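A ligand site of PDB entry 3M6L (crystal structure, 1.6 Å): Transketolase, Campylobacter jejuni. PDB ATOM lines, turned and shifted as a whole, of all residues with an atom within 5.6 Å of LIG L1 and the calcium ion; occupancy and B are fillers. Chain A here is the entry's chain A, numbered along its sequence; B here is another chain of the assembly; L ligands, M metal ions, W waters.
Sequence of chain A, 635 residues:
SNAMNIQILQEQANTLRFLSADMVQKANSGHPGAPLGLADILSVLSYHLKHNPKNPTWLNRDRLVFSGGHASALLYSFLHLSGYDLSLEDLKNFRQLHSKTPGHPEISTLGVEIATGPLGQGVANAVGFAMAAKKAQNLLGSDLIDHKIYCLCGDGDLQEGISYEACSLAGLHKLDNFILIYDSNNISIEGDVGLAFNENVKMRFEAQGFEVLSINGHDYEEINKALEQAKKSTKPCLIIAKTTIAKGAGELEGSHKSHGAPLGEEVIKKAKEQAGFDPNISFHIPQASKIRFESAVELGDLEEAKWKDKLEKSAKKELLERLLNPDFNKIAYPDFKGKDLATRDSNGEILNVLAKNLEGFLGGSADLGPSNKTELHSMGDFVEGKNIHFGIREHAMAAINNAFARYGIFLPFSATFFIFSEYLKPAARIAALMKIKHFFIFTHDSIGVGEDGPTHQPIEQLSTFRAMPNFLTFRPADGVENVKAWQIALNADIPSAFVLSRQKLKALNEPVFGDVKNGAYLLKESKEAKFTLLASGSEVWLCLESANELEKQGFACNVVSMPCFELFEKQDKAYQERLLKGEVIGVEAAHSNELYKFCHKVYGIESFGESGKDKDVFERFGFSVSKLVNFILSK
The backbone NH of Asp 155 is in hydrogen-bond range of an oxygen (O2) of LIG L1, 3.3 Å away. ND1 of His 259 is in hydrogen-bond range of O7 of LIG L1 (2.5 Å). A nitrogen (N1) of LIG L1 lies within hydrogen-bond range of the side-chain carboxylate of Glu 394 of chain B, at 2.5 Å. N3 of LIG L1 lies within hydrogen-bond range of O of Gly 117. The backbone NH (N) of Gly 156 lies within hydrogen-bond range of an oxygen (O2) of LIG L1 (2.9 Å). N of Leu 119 lies within hydrogen-bond range of N2 of LIG L1, at 3.0 Å. An oxygen (O2) of LG2 L2 lies within hydrogen-bond range of a ring nitrogen (NE2) of His 259, at 3.0 Å.
N3 of LIG L1 sits close to O1 of LG2 L2 (3.5 Å).
OE1 of Glu 394 of chain B sits close to OE2 of Glu 160 (2.5 Å). OH of Tyr 423 of chain B lies within hydrogen-bond range of O of Leu 119, 2.7 Å away. The side-chain carboxylate (OD2) of Asp 367 of chain B is in hydrogen-bond range of the backbone NH (N) of Ile 189 (3.1 Å). The side-chain hydroxyl (OG) of Ser 188 is in hydrogen-bond range of the side-chain carboxylate (OD1) of Asp 367 of chain B (2.6 Å). N of Glu 160 sits close to O of Ile 392 of chain B (3.5 Å). N of Gly 154 is in hydrogen-bond range of OD2 of Asp 157, 3.0 Å away.
Ala 34 touches LIG L1 (CB to O5, 3.2 Å). His 70 touches LIG L1. Pro 118 touches LIG L1 (CA to N2, 3.7 Å). Gly 154 touches LIG L1. Glu 160 touches LIG L1 (OE2 to C2, 3.3 Å). CB of Ser 188 touches C12 of LIG L1, 3.97 Å away. CD1 of Ile 189 touches C9 of LIG L1, 3.7 Å away. Ile 245 touches LIG L1 (CD1 to O7, 3.6 Å). Asp 367 of chain B touches LIG L1. Ile 392 of chain B touches LIG L1. Phe 420 of chain B touches LIG L1. Tyr 423 of chain B touches LIG L1. His 456 of chain B touches LIG L1 (CE1 to N3, 3.7 Å). Hydrophobic or aromatic side chains that line LIG L1: Ala 34, His 70, Leu 119, Ile 189, Ile 245, His 259, Ile 392 of chain B, Phe 420 of chain B, Tyr 423 of chain B and His 456 of chain B. Of the 30 residues printed, 21 come within 4 Å of LIG L1. Along chain A the residues within 4 Å of LIG L1 span positions 34 to 259. The nearest printed residue that does not touch LIG L1 is Leu 368 of chain B (4.1 Å).
Of the 30 residues printed, 3 come within 4 Å of the calcium ion. The nearest printed residue that does not touch the calcium ion is Ser 188 (4.5 Å).
The calcium ion is bound by an oxygen (O6) of LIG L1, an oxygen (O3) of LIG L1, the side-chain carboxylate of Asp 155, the side-chain amide oxygen of Asn 185, the backbone carbonyl oxygen of Ile 187 and water W1.
Water W1 bridges the backbone carbonyl oxygen (O) of Asp 183 (2.7 Å) and the backbone NH (N) of Asp 155 (3.2 Å). Water W4 lies within hydrogen-bond range of O2 of LIG L1 (2.7 Å), OD2 of Asp 157 (3.0 Å) and NE2 of His 70 (3.1 Å). Water W3 bridges OD2 of Asp 183 and O5 of LIG L1. Water W2 lies within hydrogen-bond range of the side-chain carboxylate (OE2) of Glu 394 of chain B (2.6 Å), the side-chain hydroxyl (OG1) of Thr 416 of chain B (2.7 Å) and the backbone carbonyl oxygen (O) of Ala 366 of chain B (2.8 Å). Water W5 lies within hydrogen-bond range of O of His 259 (2.7 Å), N of Ala 34 (2.9 Å) and O5 of LIG L1 (3.3 Å).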
ATOM      1  N   GLY A  33      20.140 -23.093   3.489  1.00  0.00           N
ATOM      2  CA  GLY A  33      19.754 -21.704   3.861  1.00  0.00           C
ATOM      3  C   GLY A  33      20.180 -21.241   5.234  1.00  0.00           C
ATOM      4  O   GLY A  33      20.791 -20.196   5.412  1.00  0.00           O
ATOM      5  N   ALA A  34      19.902 -22.077   6.239  1.00  0.00           N
ATOM      6  CA  ALA A  34      20.272 -21.740   7.613  1.00  0.00           C
ATOM      7  C   ALA A  34      21.768 -21.722   7.807  1.00  0.00           C
ATOM      8  O   ALA A  34      22.320 -20.796   8.443  1.00  0.00           O
ATOM      9  CB  ALA A  34      19.611 -22.671   8.634  1.00  0.00           C
ATOM     10  N   HIS A  70      18.220 -28.901  11.366  1.00  0.00           N
ATOM     11  CA  HIS A  70      18.400 -28.919   9.916  1.00  0.00           C
ATOM     12  C   HIS A  70      19.619 -28.149   9.487  1.00  0.00           C
ATOM     13  O   HIS A  70      20.020 -28.304   8.319  1.00  0.00           O
ATOM     14  CB  HIS A  70      17.152 -28.392   9.197  1.00  0.00           C
ATOM     15  CG  HIS A  70      16.746 -27.047   9.664  1.00  0.00           C
ATOM     16  ND1 HIS A  70      16.975 -25.915   8.945  1.00  0.00           N
ATOM     17  CD2 HIS A  70      16.193 -26.656  10.826  1.00  0.00           C
ATOM     18  CE1 HIS A  70      16.576 -24.865   9.646  1.00  0.00           C
ATOM     19  NE2 HIS A  70      16.096 -25.280  10.800  1.00  0.00           N
ATOM     20  N   GLY A 117      16.287 -31.746  15.801  1.00  0.00           N
ATOM     21  CA  GLY A 117      15.508 -32.215  14.622  1.00  0.00           C
ATOM     22  C   GLY A 117      14.026 -31.879  14.812  1.00  0.00           C
ATOM     23  O   GLY A 117      13.483 -31.166  14.019  1.00  0.00           O
ATOM     24  N   PRO A 118      13.448 -32.243  15.918  1.00  0.00           N
ATOM     25  CA  PRO A 118      12.094 -31.819  16.220  1.00  0.00           C
ATOM     26  C   PRO A 118      12.183 -30.435  16.798  1.00  0.00           C
ATOM     27  O   PRO A 118      12.852 -30.209  17.808  1.00  0.00           O
ATOM     28  CB  PRO A 118      11.614 -32.837  17.251  1.00  0.00           C
ATOM     29  CG  PRO A 118      12.563 -33.990  17.042  1.00  0.00           C
ATOM     30  CD  PRO A 118      13.845 -33.420  16.728  1.00  0.00           C
ATOM     31  N   LEU A 119      11.529 -29.482  16.192  1.00  0.00           N
ATOM     32  CA  LEU A 119      11.758 -28.090  16.553  1.00  0.00           C
ATOM     33  C   LEU A 119      11.257 -27.785  17.942  1.00  0.00           C
ATOM     34  O   LEU A 119      10.265 -28.404  18.511  1.00  0.00           O
ATOM     35  CB  LEU A 119      11.104 -27.193  15.541  1.00  0.00           C
ATOM     36  CG  LEU A 119      11.769 -27.154  14.165  1.00  0.00           C
ATOM     37  CD1 LEU A 119      10.748 -26.537  13.159  1.00  0.00           C
ATOM     38  CD2 LEU A 119      13.035 -26.294  14.206  1.00  0.00           C
ATOM     39  N   GLY A 154      15.710 -20.854  15.415  1.00  0.00           N
ATOM     40  CA  GLY A 154      15.104 -20.117  14.344  1.00  0.00           C
ATOM     41  C   GLY A 154      13.643 -19.837  14.666  1.00  0.00           C
ATOM     42  O   GLY A 154      13.151 -20.063  15.741  1.00  0.00           O
ATOM     43  N   ASP A 155      12.956 -19.371  13.633  1.00  0.00           N
ATOM     44  CA  ASP A 155      11.470 -19.085  13.693  1.00  0.00           C
ATOM     45  C   ASP A 155      10.697 -20.267  14.158  1.00  0.00           C
ATOM     46  O   ASP A 155       9.749 -20.133  14.955  1.00  0.00           O
ATOM     47  CB  ASP A 155      10.970 -18.671  12.330  1.00  0.00           C
ATOM     48  CG  ASP A 155      11.623 -17.335  11.895  1.00  0.00           C
ATOM     49  OD1 ASP A 155      11.474 -16.307  12.593  1.00  0.00           O
ATOM     50  OD2 ASP A 155      12.329 -17.278  10.875  1.00  0.00           O
ATOM     51  N   GLY A 156      11.014 -21.393  13.610  1.00  0.00           N
ATOM     52  CA  GLY A 156      10.307 -22.600  13.866  1.00  0.00           C
ATOM     53  C   GLY A 156      10.374 -22.980  15.362  1.00  0.00           C
ATOM     54  O   GLY A 156       9.362 -23.381  15.989  1.00  0.00           O
ATOM     55  N   ASP A 157      11.550 -22.858  15.920  1.00  0.00           N
ATOM     56  CA  ASP A 157      11.703 -23.177  17.352  1.00  0.00           C
ATOM     57  C   ASP A 157      10.803 -22.265  18.229  1.00  0.00           C
ATOM     58  O   ASP A 157      10.232 -22.694  19.232  1.00  0.00           O
ATOM     59  CB  ASP A 157      13.130 -23.006  17.788  1.00  0.00           C
ATOM     60  CG  ASP A 157      14.064 -23.979  17.122  1.00  0.00           C
ATOM     61  OD1 ASP A 157      13.975 -25.194  17.436  1.00  0.00           O
ATOM     62  OD2 ASP A 157      14.886 -23.558  16.282  1.00  0.00           O
ATOM     63  N   GLU A 160       6.954 -22.917  18.477  1.00  0.00           N
ATOM     64  CA  GLU A 160       6.538 -24.125  19.250  1.00  0.00           C
ATOM     65  C   GLU A 160       6.295 -23.802  20.694  1.00  0.00           C
ATOM     66  O   GLU A 160       7.120 -23.117  21.340  1.00  0.00           O
ATOM     67  CB  GLU A 160       7.556 -25.241  19.135  1.00  0.00           C
ATOM     68  CG  GLU A 160       7.606 -25.887  17.815  1.00  0.00           C
ATOM     69  CD  GLU A 160       6.455 -26.874  17.586  1.00  0.00           C
ATOM     70  OE1 GLU A 160       5.619 -27.029  18.502  1.00  0.00           O
ATOM     71  OE2 GLU A 160       6.400 -27.464  16.442  1.00  0.00           O
ATOM     72  N   ASP A 183      17.966 -16.655  15.067  1.00  0.00           N
ATOM     73  CA  ASP A 183      18.175 -16.357  13.659  1.00  0.00           C
ATOM     74  C   ASP A 183      16.858 -15.884  13.075  1.00  0.00           C
ATOM     75  O   ASP A 183      16.030 -16.667  12.595  1.00  0.00           O
ATOM     76  CB  ASP A 183      18.655 -17.639  12.936  1.00  0.00           C
ATOM     77  CG  ASP A 183      19.045 -17.419  11.488  1.00  0.00           C
ATOM     78  OD1 ASP A 183      19.300 -16.225  11.114  1.00  0.00           O
ATOM     79  OD2 ASP A 183      19.080 -18.438  10.704  1.00  0.00           O
ATOM     80  N   ASN A 185      15.300 -14.503  10.168  1.00  0.00           N
ATOM     81  CA  ASN A 185      15.435 -14.315   8.744  1.00  0.00           C
ATOM     82  C   ASN A 185      14.117 -14.079   7.927  1.00  0.00           C
ATOM     83  O   ASN A 185      14.126 -13.990   6.643  1.00  0.00           O
ATOM     84  CB  ASN A 185      16.306 -15.424   8.149  1.00  0.00           C
ATOM     85  CG  ASN A 185      15.629 -16.784   8.194  1.00  0.00           C
ATOM     86  OD1 ASN A 185      14.409 -16.886   8.413  1.00  0.00           O
ATOM     87  ND2 ASN A 185      16.456 -17.890   8.048  1.00  0.00           N
ATOM     88  N   ASN A 186      12.989 -13.968   8.635  1.00  0.00           N
ATOM     89  CA  ASN A 186      11.701 -13.685   8.069  1.00  0.00           C
ATOM     90  C   ASN A 186      11.199 -14.716   7.099  1.00  0.00           C
ATOM     91  O   ASN A 186      10.265 -14.438   6.407  1.00  0.00           O
ATOM     92  CB  ASN A 186      11.717 -12.301   7.350  1.00  0.00           C
ATOM     93  CG  ASN A 186      10.312 -11.688   7.230  1.00  0.00           C
ATOM     94  OD1 ASN A 186       9.976 -11.154   6.186  1.00  0.00           O
ATOM     95  ND2 ASN A 186       9.513 -11.780   8.288  1.00  0.00           N
ATOM     96  N   ILE A 187      11.799 -15.916   7.086  1.00  0.00           N
ATOM     97  CA  ILE A 187      11.396 -16.960   6.120  1.00  0.00           C
ATOM     98  C   ILE A 187      11.150 -18.296   6.784  1.00  0.00           C
ATOM     99  O   ILE A 187      11.855 -18.641   7.696  1.00  0.00           O
ATOM    100  CB  ILE A 187      12.524 -17.155   5.053  1.00  0.00           C
ATOM    101  CG1 ILE A 187      12.568 -15.877   4.153  1.00  0.00           C
ATOM    102  CG2 ILE A 187      12.353 -18.539   4.285  1.00  0.00           C
ATOM    103  CD1 ILE A 187      11.568 -15.881   3.050  1.00  0.00           C
ATOM    104  N   SER A 188      10.102 -19.007   6.355  1.00  0.00           N
ATOM    105  CA  SER A 188       9.921 -20.429   6.748  1.00  0.00           C
ATOM    106  C   SER A 188       9.542 -21.173   5.559  1.00  0.00           C
ATOM    107  O   SER A 188       9.615 -20.654   4.467  1.00  0.00           O
ATOM    108  CB  SER A 188       8.861 -20.538   7.873  1.00  0.00           C
ATOM    109  OG  SER A 188       7.560 -20.192   7.491  1.00  0.00           O
ATOM    110  N   ILE A 189       9.144 -22.441   5.691  1.00  0.00           N
ATOM    111  CA  ILE A 189       8.938 -23.263   4.523  1.00  0.00           C
ATOM    112  C   ILE A 189       7.783 -22.729   3.630  1.00  0.00           C
ATOM    113  O   ILE A 189       7.846 -22.810   2.406  1.00  0.00           O
ATOM    114  CB  ILE A 189       8.636 -24.719   4.976  1.00  0.00           C
ATOM    115  CG1 ILE A 189       9.882 -25.310   5.643  1.00  0.00           C
ATOM    116  CG2 ILE A 189       8.109 -25.530   3.811  1.00  0.00           C
ATOM    117  CD1 ILE A 189       9.718 -26.798   6.116  1.00  0.00           C
ATOM    118  N   VAL A 193       7.457 -15.213   7.125  1.00  0.00           N
ATOM    119  CA  VAL A 193       7.062 -15.533   8.505  1.00  0.00           C
ATOM    120  C   VAL A 193       5.792 -14.789   8.900  1.00  0.00           C
ATOM    121  O   VAL A 193       4.980 -15.257   9.651  1.00  0.00           O
ATOM    122  CB  VAL A 193       8.215 -15.279   9.452  1.00  0.00           C
ATOM    123  CG1 VAL A 193       7.784 -15.194  10.943  1.00  0.00           C
ATOM    124  CG2 VAL A 193       9.266 -16.430   9.280  1.00  0.00           C
ATOM    125  N   ILE A 245      18.344 -15.440   4.918  1.00  0.00           N
ATOM    126  CA  ILE A 245      18.497 -16.873   4.627  1.00  0.00           C
ATOM    127  C   ILE A 245      19.363 -17.052   3.358  1.00  0.00           C
ATOM    128  O   ILE A 245      19.241 -16.286   2.407  1.00  0.00           O
ATOM    129  CB  ILE A 245      17.122 -17.614   4.569  1.00  0.00           C
ATOM    130  CG1 ILE A 245      17.373 -19.134   4.596  1.00  0.00           C
ATOM    131  CG2 ILE A 245      16.407 -17.283   3.321  1.00  0.00           C
ATOM    132  CD1 ILE A 245      16.064 -19.943   4.778  1.00  0.00           C
ATOM    133  N   HIS A 259      15.547 -23.061   1.920  1.00  0.00           N
ATOM    134  CA  HIS A 259      15.432 -23.705   3.245  1.00  0.00           C
ATOM    135  C   HIS A 259      15.933 -25.137   3.227  1.00  0.00           C
ATOM    136  O   HIS A 259      16.681 -25.550   4.146  1.00  0.00           O
ATOM    137  CB  HIS A 259      13.964 -23.650   3.763  1.00  0.00           C
ATOM    138  CG  HIS A 259      13.729 -24.602   4.878  1.00  0.00           C
ATOM    139  ND1 HIS A 259      14.155 -24.335   6.137  1.00  0.00           N
ATOM    140  CD2 HIS A 259      13.292 -25.887   4.897  1.00  0.00           C
ATOM    141  CE1 HIS A 259      13.930 -25.387   6.929  1.00  0.00           C
ATOM    142  NE2 HIS A 259      13.419 -26.353   6.194  1.00  0.00           N
ATOM    143  N   ALA B 366       0.939 -27.138   9.533  1.00  0.00           N
ATOM    144  CA  ALA B 366       1.844 -26.496  10.433  1.00  0.00           C
ATOM    145  C   ALA B 366       3.189 -26.163   9.773  1.00  0.00           C
ATOM    146  O   ALA B 366       4.205 -26.857   9.954  1.00  0.00           O
ATOM    147  CB  ALA B 366       2.041 -27.301  11.741  1.00  0.00           C
ATOM    148  N   ASP B 367       3.153 -25.158   8.920  1.00  0.00           N
ATOM    149  CA  ASP B 367       4.301 -24.698   8.075  1.00  0.00           C
ATOM    150  C   ASP B 367       4.820 -25.676   7.028  1.00  0.00           C
ATOM    151  O   ASP B 367       5.929 -25.463   6.538  1.00  0.00           O
ATOM    152  CB  ASP B 367       5.438 -24.121   8.936  1.00  0.00           C
ATOM    153  CG  ASP B 367       6.483 -23.282   8.108  1.00  0.00           C
ATOM    154  OD1 ASP B 367       6.076 -22.361   7.315  1.00  0.00           O
ATOM    155  OD2 ASP B 367       7.719 -23.529   8.195  1.00  0.00           O
ATOM    156  N   LEU B 368       4.097 -26.738   6.669  1.00  0.00           N
ATOM    157  CA  LEU B 368       4.610 -27.752   5.788  1.00  0.00           C
ATOM    158  C   LEU B 368       3.734 -27.925   4.561  1.00  0.00           C
ATOM    159  O   LEU B 368       3.783 -28.951   3.867  1.00  0.00           O
ATOM    160  CB  LEU B 368       4.708 -29.098   6.489  1.00  0.00           C
ATOM    161  CG  LEU B 368       5.865 -29.155   7.463  1.00  0.00           C
ATOM    162  CD1 LEU B 368       5.875 -30.411   8.376  1.00  0.00           C
ATOM    163  CD2 LEU B 368       7.198 -29.116   6.672  1.00  0.00           C
ATOM    164  N   ILE B 392       4.422 -23.043  12.972  1.00  0.00           N
ATOM    165  CA  ILE B 392       5.014 -24.259  13.555  1.00  0.00           C
ATOM    166  C   ILE B 392       4.355 -24.492  14.919  1.00  0.00           C
ATOM    167  O   ILE B 392       5.001 -24.311  15.973  1.00  0.00           O
ATOM    168  CB  ILE B 392       6.546 -24.198  13.583  1.00  0.00           C
ATOM    169  CG1 ILE B 392       7.187 -23.942  12.214  1.00  0.00           C
ATOM    170  CG2 ILE B 392       7.091 -25.605  13.933  1.00  0.00           C
ATOM    171  CD1 ILE B 392       7.211 -22.433  11.719  1.00  0.00           C
ATOM    172  N   GLU B 394       1.855 -27.380  15.814  1.00  0.00           N
ATOM    173  CA  GLU B 394       1.054 -28.555  15.581  1.00  0.00           C
ATOM    174  C   GLU B 394      -0.063 -28.672  16.615  1.00  0.00           C
ATOM    175  O   GLU B 394      -1.196 -29.038  16.258  1.00  0.00           O
ATOM    176  CB  GLU B 394       1.898 -29.828  15.568  1.00  0.00           C
ATOM    177  CG  GLU B 394       2.917 -29.902  14.474  1.00  0.00           C
ATOM    178  CD  GLU B 394       4.228 -29.214  14.778  1.00  0.00           C
ATOM    179  OE1 GLU B 394       4.369 -28.765  15.967  1.00  0.00           O
ATOM    180  OE2 GLU B 394       5.106 -29.221  13.884  1.00  0.00           O
ATOM    181  N   THR B 416       0.537 -32.326   9.089  1.00  0.00           N
ATOM    182  CA  THR B 416       1.949 -32.293   9.380  1.00  0.00           C
ATOM    183  C   THR B 416       2.592 -33.611   8.930  1.00  0.00           C
ATOM    184  O   THR B 416       1.930 -34.482   8.358  1.00  0.00           O
ATOM    185  CB  THR B 416       2.259 -31.944  10.911  1.00  0.00           C
ATOM    186  OG1 THR B 416       3.663 -31.771  11.104  1.00  0.00           O
ATOM    187  CG2 THR B 416       1.536 -33.037  11.724  1.00  0.00           C
ATOM    188  N   PHE B 417       3.896 -33.697   9.164  1.00  0.00           N
ATOM    189  CA  PHE B 417       4.598 -34.957   8.935  1.00  0.00           C
ATOM    190  C   PHE B 417       4.088 -35.903   9.989  1.00  0.00           C
ATOM    191  O   PHE B 417       3.868 -35.507  11.161  1.00  0.00           O
ATOM    192  CB  PHE B 417       6.124 -34.817   9.047  1.00  0.00           C
ATOM    193  CG  PHE B 417       6.821 -34.012   8.023  1.00  0.00           C
ATOM    194  CD1 PHE B 417       6.334 -33.939   6.733  1.00  0.00           C
ATOM    195  CD2 PHE B 417       8.020 -33.333   8.340  1.00  0.00           C
ATOM    196  CE1 PHE B 417       7.076 -33.220   5.815  1.00  0.00           C
ATOM    197  CE2 PHE B 417       8.696 -32.653   7.407  1.00  0.00           C
ATOM    198  CZ  PHE B 417       8.208 -32.617   6.162  1.00  0.00           C
ATOM    199  N   PHE B 420       5.521 -35.857  13.509  1.00  0.00           N
ATOM    200  CA  PHE B 420       5.100 -34.741  14.384  1.00  0.00           C
ATOM    201  C   PHE B 420       3.616 -34.754  14.769  1.00  0.00           C
ATOM    202  O   PHE B 420       3.106 -33.871  15.455  1.00  0.00           O
ATOM    203  CB  PHE B 420       5.595 -33.393  13.815  1.00  0.00           C
ATOM    204  CG  PHE B 420       7.106 -33.356  13.515  1.00  0.00           C
ATOM    205  CD1 PHE B 420       8.022 -33.790  14.423  1.00  0.00           C
ATOM    206  CD2 PHE B 420       7.570 -32.959  12.297  1.00  0.00           C
ATOM    207  CE1 PHE B 420       9.410 -33.783  14.153  1.00  0.00           C
ATOM    208  CE2 PHE B 420       8.920 -32.938  12.030  1.00  0.00           C
ATOM    209  CZ  PHE B 420       9.800 -33.416  12.923  1.00  0.00           C
ATOM    210  N   TYR B 423       3.292 -34.219  18.455  1.00  0.00           N
ATOM    211  CA  TYR B 423       3.120 -32.888  19.002  1.00  0.00           C
ATOM    212  C   TYR B 423       1.620 -32.523  19.158  1.00  0.00           C
ATOM    213  O   TYR B 423       1.335 -31.689  20.021  1.00  0.00           O
ATOM    214  CB  TYR B 423       3.816 -31.852  18.190  1.00  0.00           C
ATOM    215  CG  TYR B 423       5.276 -31.638  18.399  1.00  0.00           C
ATOM    216  CD1 TYR B 423       6.229 -32.620  18.086  1.00  0.00           C
ATOM    217  CD2 TYR B 423       5.795 -30.433  18.921  1.00  0.00           C
ATOM    218  CE1 TYR B 423       7.558 -32.445  18.201  1.00  0.00           C
ATOM    219  CE2 TYR B 423       7.148 -30.233  19.050  1.00  0.00           C
ATOM    220  CZ  TYR B 423       8.050 -31.233  18.766  1.00  0.00           C
ATOM    221  OH  TYR B 423       9.388 -30.975  18.865  1.00  0.00           O
ATOM    222  N   HIS B 456      13.036 -38.029  12.063  1.00  0.00           N
ATOM    223  CA  HIS B 456      11.984 -37.772  11.098  1.00  0.00           C
ATOM    224  C   HIS B 456      11.354 -39.035  10.519  1.00  0.00           C
ATOM    225  O   HIS B 456      10.574 -38.880   9.579  1.00  0.00           O
ATOM    226  CB  HIS B 456      12.532 -36.890   9.971  1.00  0.00           C
ATOM    227  CG  HIS B 456      12.800 -35.480  10.435  1.00  0.00           C
ATOM    228  ND1 HIS B 456      12.346 -34.351   9.781  1.00  0.00           N
ATOM    229  CD2 HIS B 456      13.456 -35.060  11.519  1.00  0.00           C
ATOM    230  CE1 HIS B 456      12.747 -33.284  10.487  1.00  0.00           C
ATOM    231  NE2 HIS B 456      13.429 -33.709  11.527  1.00  0.00           N
HETATM  232  N1  LIG L   1       7.535 -29.557  13.315  1.00  0.00           N
HETATM  233  C1  LIG L   1       8.529 -29.894  14.136  1.00  0.00           C
HETATM  234  C2  LIG L   1       8.163 -30.089  15.598  1.00  0.00           C
HETATM  235  N2  LIG L   1       9.829 -30.094  13.823  1.00  0.00           N
HETATM  236  C3  LIG L   1      10.189 -30.030  12.542  1.00  0.00           C
HETATM  237  N3  LIG L   1      11.453 -30.292  12.260  1.00  0.00           N
HETATM  238  C4  LIG L   1       9.164 -29.617  11.532  1.00  0.00           C
HETATM  239  C5  LIG L   1       7.863 -29.410  11.989  1.00  0.00           C
HETATM  240  C6  LIG L   1       9.535 -29.433  10.008  1.00  0.00           C
HETATM  241  N4  LIG L   1      10.406 -28.159   9.839  1.00  0.00           N
HETATM  242  C7  LIG L   1      11.784 -28.003   9.787  1.00  0.00           C
HETATM  243  S1  LIG L   1      12.495 -26.374   9.755  1.00  0.00           S
HETATM  244  C8  LIG L   1      10.835 -25.797   9.678  1.00  0.00           C
HETATM  245  C9  LIG L   1       9.879 -26.905   9.777  1.00  0.00           C
HETATM  246  C10 LIG L   1       8.439 -26.584   9.841  1.00  0.00           C
HETATM  247  C11 LIG L   1      10.421 -24.346   9.575  1.00  0.00           C
HETATM  248  C12 LIG L   1      11.421 -23.335   9.042  1.00  0.00           C
HETATM  249  O1  LIG L   1      12.018 -23.040  10.239  1.00  0.00           O
HETATM  250  P1  LIG L   1      13.073 -22.004  10.622  1.00  0.00           P
HETATM  251  O2  LIG L   1      13.260 -22.286  12.049  1.00  0.00           O
HETATM  252  O3  LIG L   1      12.481 -20.653  10.274  1.00  0.00           O
HETATM  253  O4  LIG L   1      14.280 -22.354   9.688  1.00  0.00           O
HETATM  254  P2  LIG L   1      15.105 -21.660   8.488  1.00  0.00           P
HETATM  255  O5  LIG L   1      16.483 -22.118   8.686  1.00  0.00           O
HETATM  256  O6  LIG L   1      14.880 -20.177   8.474  1.00  0.00           O
HETATM  257  O7  LIG L   1      14.494 -22.113   7.204  1.00  0.00           O
HETATM  258  C1  LG2 L   2      12.437 -30.932   8.503  1.00  0.00           C
HETATM  259  O1  LG2 L   2      13.478 -30.519   9.450  1.00  0.00           O
HETATM  260  C2  LG2 L   2      12.779 -30.522   7.059  1.00  0.00           C
HETATM  261  O2  LG2 L   2      12.495 -29.147   6.755  1.00  0.00           O
HETATM  262  C3  LG2 L   2      12.329 -31.457   5.900  1.00  0.00           C
HETATM  263  O3  LG2 L   2      13.641 -31.876   5.549  1.00  0.00           O
HETATM  264  C4  LG2 L   2      11.828 -30.956   4.511  1.00  0.00           C
HETATM  265  O4  LG2 L   2      10.979 -29.800   4.677  1.00  0.00           O
HETATM  266  C5  LG2 L   2      11.217 -32.071   3.581  1.00  0.00           C
HETATM  267  O5  LG2 L   2      11.262 -31.854   2.114  1.00  0.00           O
HETATM  268  P1  LG2 L   2      10.460 -32.819   1.044  1.00  0.00           P
HETATM  269  O6  LG2 L   2       9.020 -32.180   0.605  1.00  0.00           O
HETATM  270  O7  LG2 L   2      10.312 -34.189   1.902  1.00  0.00           O
HETATM  271  O8  LG2 L   2      11.201 -33.211  -0.196  1.00  0.00           O
HETATM  272 CA    CA M   1      13.406 -18.725   9.444  1.00  0.00          CA
HETATM  273  O   HOH W   1      14.973 -18.698  11.251  1.00  0.00           O
HETATM  274  O   HOH W   2       4.672 -29.278  11.301  1.00  0.00           O
HETATM  275  O   HOH W   3      17.261 -20.411  10.970  1.00  0.00           O
HETATM  276  O   HOH W   4      15.236 -23.603  13.258  1.00  0.00           O
HETATM  277  O   HOH W   5      17.590 -23.857   6.097  1.00  0.00           O
